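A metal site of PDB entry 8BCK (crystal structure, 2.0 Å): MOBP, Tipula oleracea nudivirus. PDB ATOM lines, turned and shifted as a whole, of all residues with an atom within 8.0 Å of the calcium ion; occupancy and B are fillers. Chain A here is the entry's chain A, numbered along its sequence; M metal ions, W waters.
The calcium ion is bound by the backbone carbonyl oxygen (O) of Asn 148 (2.3 Å), the backbone carbonyl oxygen (O) of Asp 140 (2.4 Å), water W2 (2.4 Å), the side-chain carboxylate (OD1) of Asp 140 (2.5 Å), the side-chain amide oxygen (OD1) of Asn 143 (2.5 Å), water W1 (2.6 Å) and the side-chain amide nitrogen (ND2) of Asn 143 (2.9 Å).
Three residues have an atom within 4 Å of the calcium ion: Asp 140, Asn 143 and Asn 148.
Water W1 lies within hydrogen-bond range of OG1 of Thr 144 (2.9 Å), N of Asn 148 (3.0 Å), O of Phe 141 (3.0 Å) and O of Trp 146 (3.0 Å).
The side-chain carboxylate (OD2) of Asp 140 lies within hydrogen-bond range of the backbone NH (N) of Ser 150 (2.9 Å).
The side-chain carboxylate (OD2) of Asp 140 is in hydrogen-bond range of a ring nitrogen (ND1) of His 153, at 2.7 Å.
The side-chain hydroxyl (OG1) of Thr 144 lies close to the side-chain amide oxygen (OD1) of Asn 143 (3.3 Å).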
ATOM      1  N   LEU A 137      25.841  12.059 -15.707  1.00  0.00           N
ATOM      2  CA  LEU A 137      25.526  12.520 -14.363  1.00  0.00           C
ATOM      3  C   LEU A 137      26.519  11.982 -13.343  1.00  0.00           C
ATOM      4  O   LEU A 137      27.062  12.737 -12.526  1.00  0.00           O
ATOM      5  CB  LEU A 137      24.097  12.090 -13.992  1.00  0.00           C
ATOM      6  CG  LEU A 137      23.767  12.004 -12.507  1.00  0.00           C
ATOM      7  CD1 LEU A 137      23.738  13.384 -11.881  1.00  0.00           C
ATOM      8  CD2 LEU A 137      22.419  11.310 -12.287  1.00  0.00           C
ATOM      9  N   ILE A 138      26.778  10.671 -13.384  1.00  0.00           N
ATOM     10  CA  ILE A 138      27.685  10.068 -12.401  1.00  0.00           C
ATOM     11  C   ILE A 138      29.065  10.702 -12.498  1.00  0.00           C
ATOM     12  O   ILE A 138      29.711  10.988 -11.471  1.00  0.00           O
ATOM     13  CB  ILE A 138      27.764   8.546 -12.614  1.00  0.00           C
ATOM     14  CG1 ILE A 138      26.402   7.895 -12.305  1.00  0.00           C
ATOM     15  CG2 ILE A 138      28.842   7.944 -11.729  1.00  0.00           C
ATOM     16  CD1 ILE A 138      26.187   6.578 -13.033  1.00  0.00           C
ATOM     17  N   CYS A 139      29.563  10.924 -13.719  1.00  0.00           N
ATOM     18  CA  CYS A 139      30.870  11.549 -13.890  1.00  0.00           C
ATOM     19  C   CYS A 139      30.905  12.935 -13.256  1.00  0.00           C
ATOM     20  O   CYS A 139      31.897  13.318 -12.628  1.00  0.00           O
ATOM     21  CB  CYS A 139      31.210  11.627 -15.380  1.00  0.00           C
ATOM     22  SG  CYS A 139      31.615  10.006 -16.135  1.00  0.00           S
ATOM     23  N   ASP A 140      29.836  13.710 -13.427  1.00  0.00           N
ATOM     24  CA  ASP A 140      29.783  15.036 -12.823  1.00  0.00           C
ATOM     25  C   ASP A 140      29.763  14.931 -11.293  1.00  0.00           C
ATOM     26  O   ASP A 140      30.460  15.676 -10.606  1.00  0.00           O
ATOM     27  CB  ASP A 140      28.546  15.781 -13.330  1.00  0.00           C
ATOM     28  CG  ASP A 140      28.406  17.194 -12.748  1.00  0.00           C
ATOM     29  OD1 ASP A 140      29.300  17.635 -11.994  1.00  0.00           O
ATOM     30  OD2 ASP A 140      27.402  17.862 -13.070  1.00  0.00           O
ATOM     31  N   PHE A 141      28.988  13.987 -10.762  1.00  0.00           N
ATOM     32  CA  PHE A 141      28.904  13.827  -9.305  1.00  0.00           C
ATOM     33  C   PHE A 141      30.263  13.553  -8.694  1.00  0.00           C
ATOM     34  O   PHE A 141      30.565  14.034  -7.590  1.00  0.00           O
ATOM     35  CB  PHE A 141      27.926  12.690  -8.981  1.00  0.00           C
ATOM     36  CG  PHE A 141      27.536  12.626  -7.528  1.00  0.00           C
ATOM     37  CD1 PHE A 141      28.328  11.929  -6.618  1.00  0.00           C
ATOM     38  CD2 PHE A 141      26.380  13.231  -7.079  1.00  0.00           C
ATOM     39  CE1 PHE A 141      27.964  11.841  -5.284  1.00  0.00           C
ATOM     40  CE2 PHE A 141      26.012  13.160  -5.743  1.00  0.00           C
ATOM     41  CZ  PHE A 141      26.811  12.466  -4.845  1.00  0.00           C
ATOM     42  N   LYS A 142      31.105  12.788  -9.394  1.00  0.00           N
ATOM     43  CA  LYS A 142      32.354  12.271  -8.849  1.00  0.00           C
ATOM     44  C   LYS A 142      33.573  13.072  -9.276  1.00  0.00           C
ATOM     45  O   LYS A 142      34.694  12.696  -8.921  1.00  0.00           O
ATOM     46  CB  LYS A 142      32.521  10.807  -9.257  1.00  0.00           C
ATOM     47  CG  LYS A 142      31.690   9.835  -8.418  1.00  0.00           C
ATOM     48  CD  LYS A 142      32.174   8.391  -8.550  1.00  0.00           C
ATOM     49  CE  LYS A 142      33.212   8.029  -7.497  1.00  0.00           C
ATOM     50  NZ  LYS A 142      34.608   8.136  -8.019  1.00  0.00           N
ATOM     51  N   ASN A 143      33.396  14.166 -10.015  1.00  0.00           N
ATOM     52  CA  ASN A 143      34.530  14.973 -10.469  1.00  0.00           C
ATOM     53  C   ASN A 143      35.161  15.815  -9.368  1.00  0.00           C
ATOM     54  O   ASN A 143      36.249  16.358  -9.588  1.00  0.00           O
ATOM     55  CB  ASN A 143      34.109  15.828 -11.668  1.00  0.00           C
ATOM     56  CG  ASN A 143      33.176  16.962 -11.285  1.00  0.00           C
ATOM     57  OD1 ASN A 143      33.179  17.451 -10.153  1.00  0.00           O
ATOM     58  ND2 ASN A 143      32.376  17.417 -12.258  1.00  0.00           N
ATOM     59  N   THR A 144      34.532  15.932  -8.196  1.00  0.00           N
ATOM     60  CA  THR A 144      35.124  16.578  -7.028  1.00  0.00           C
ATOM     61  C   THR A 144      34.578  15.901  -5.772  1.00  0.00           C
ATOM     62  O   THR A 144      33.388  15.545  -5.737  1.00  0.00           O
ATOM     63  CB  THR A 144      34.805  18.081  -6.954  1.00  0.00           C
ATOM     64  OG1 THR A 144      33.387  18.288  -7.003  1.00  0.00           O
ATOM     65  CG2 THR A 144      35.480  18.838  -8.106  1.00  0.00           C
ATOM     66  N   PRO A 145      35.396  15.753  -4.721  1.00  0.00           N
ATOM     67  CA  PRO A 145      34.852  15.224  -3.459  1.00  0.00           C
ATOM     68  C   PRO A 145      33.686  16.044  -2.914  1.00  0.00           C
ATOM     69  O   PRO A 145      32.712  15.479  -2.396  1.00  0.00           O
ATOM     70  CB  PRO A 145      36.067  15.264  -2.517  1.00  0.00           C
ATOM     71  CG  PRO A 145      37.261  15.202  -3.437  1.00  0.00           C
ATOM     72  CD  PRO A 145      36.854  15.989  -4.646  1.00  0.00           C
ATOM     73  N   TRP A 146      33.778  17.365  -2.992  1.00  0.00           N
ATOM     74  CA  TRP A 146      32.629  18.222  -2.710  1.00  0.00           C
ATOM     75  C   TRP A 146      31.584  18.054  -3.810  1.00  0.00           C
ATOM     76  O   TRP A 146      31.882  18.250  -4.993  1.00  0.00           O
ATOM     77  CB  TRP A 146      33.066  19.678  -2.610  1.00  0.00           C
ATOM     78  CG  TRP A 146      31.984  20.627  -2.183  1.00  0.00           C
ATOM     79  CD1 TRP A 146      31.075  21.227  -2.996  1.00  0.00           C
ATOM     80  CD2 TRP A 146      31.715  21.083  -0.863  1.00  0.00           C
ATOM     81  NE1 TRP A 146      30.243  22.041  -2.251  1.00  0.00           N
ATOM     82  CE2 TRP A 146      30.613  21.961  -0.931  1.00  0.00           C
ATOM     83  CE3 TRP A 146      32.295  20.827   0.395  1.00  0.00           C
ATOM     84  CZ2 TRP A 146      30.085  22.604   0.190  1.00  0.00           C
ATOM     85  CZ3 TRP A 146      31.768  21.466   1.507  1.00  0.00           C
ATOM     86  CH2 TRP A 146      30.669  22.339   1.396  1.00  0.00           C
ATOM     87  N   ILE A 147      30.357  17.697  -3.421  1.00  0.00           N
ATOM     88  CA  ILE A 147      29.321  17.406  -4.404  1.00  0.00           C
ATOM     89  C   ILE A 147      28.814  18.711  -4.993  1.00  0.00           C
ATOM     90  O   ILE A 147      28.357  19.606  -4.263  1.00  0.00           O
ATOM     91  CB  ILE A 147      28.183  16.602  -3.772  1.00  0.00           C
ATOM     92  CG1 ILE A 147      28.591  15.171  -3.417  1.00  0.00           C
ATOM     93  CG2 ILE A 147      26.978  16.548  -4.728  1.00  0.00           C
ATOM     94  CD1 ILE A 147      29.799  15.043  -2.553  1.00  0.00           C
ATOM     95  N   ASN A 148      28.871  18.821  -6.317  1.00  0.00           N
ATOM     96  CA  ASN A 148      28.338  19.963  -7.044  1.00  0.00           C
ATOM     97  C   ASN A 148      27.945  19.446  -8.413  1.00  0.00           C
ATOM     98  O   ASN A 148      28.754  18.808  -9.090  1.00  0.00           O
ATOM     99  CB  ASN A 148      29.362  21.089  -7.154  1.00  0.00           C
ATOM    100  CG  ASN A 148      28.756  22.389  -7.644  1.00  0.00           C
ATOM    101  OD1 ASN A 148      27.700  22.399  -8.282  1.00  0.00           O
ATOM    102  ND2 ASN A 148      29.401  23.507  -7.325  1.00  0.00           N
ATOM    103  N   LEU A 149      26.698  19.705  -8.821  1.00  0.00           N
ATOM    104  CA  LEU A 149      26.155  19.168 -10.057  1.00  0.00           C
ATOM    105  C   LEU A 149      25.706  20.312 -10.963  1.00  0.00           C
ATOM    106  O   LEU A 149      25.213  21.332 -10.480  1.00  0.00           O
ATOM    107  CB  LEU A 149      24.974  18.246  -9.768  1.00  0.00           C
ATOM    108  CG  LEU A 149      25.299  16.892  -9.127  1.00  0.00           C
ATOM    109  CD1 LEU A 149      24.015  16.063  -8.955  1.00  0.00           C
ATOM    110  CD2 LEU A 149      26.316  16.111  -9.927  1.00  0.00           C
ATOM    111  N   SER A 150      25.864  20.135 -12.268  1.00  0.00           N
ATOM    112  CA  SER A 150      25.327  21.108 -13.216  1.00  0.00           C
ATOM    113  C   SER A 150      23.804  21.185 -13.049  1.00  0.00           C
ATOM    114  O   SER A 150      23.152  20.251 -12.549  1.00  0.00           O
ATOM    115  CB  SER A 150      25.681  20.740 -14.655  1.00  0.00           C
ATOM    116  OG  SER A 150      25.041  19.547 -15.060  1.00  0.00           O
ATOM    117  N   HIS A 153      22.271  18.180 -14.540  1.00  0.00           N
ATOM    118  CA  HIS A 153      22.488  16.921 -13.838  1.00  0.00           C
ATOM    119  C   HIS A 153      21.715  16.870 -12.529  1.00  0.00           C
ATOM    120  O   HIS A 153      21.277  15.789 -12.115  1.00  0.00           O
ATOM    121  CB  HIS A 153      23.986  16.723 -13.591  1.00  0.00           C
ATOM    122  CG  HIS A 153      24.747  16.300 -14.806  1.00  0.00           C
ATOM    123  ND1 HIS A 153      26.055  16.666 -15.030  1.00  0.00           N
ATOM    124  CD2 HIS A 153      24.377  15.544 -15.864  1.00  0.00           C
ATOM    125  CE1 HIS A 153      26.467  16.150 -16.164  1.00  0.00           C
ATOM    126  NE2 HIS A 153      25.477  15.456 -16.696  1.00  0.00           N
HETATM  127 CA    CA M   1      30.713  17.941  -9.962  1.00  0.00          CA
HETATM  128  O   HOH W   1      30.862  17.020  -7.572  1.00  0.00           O
HETATM  129  O   HOH W   2      32.244  19.493  -8.854  1.00  0.00           O
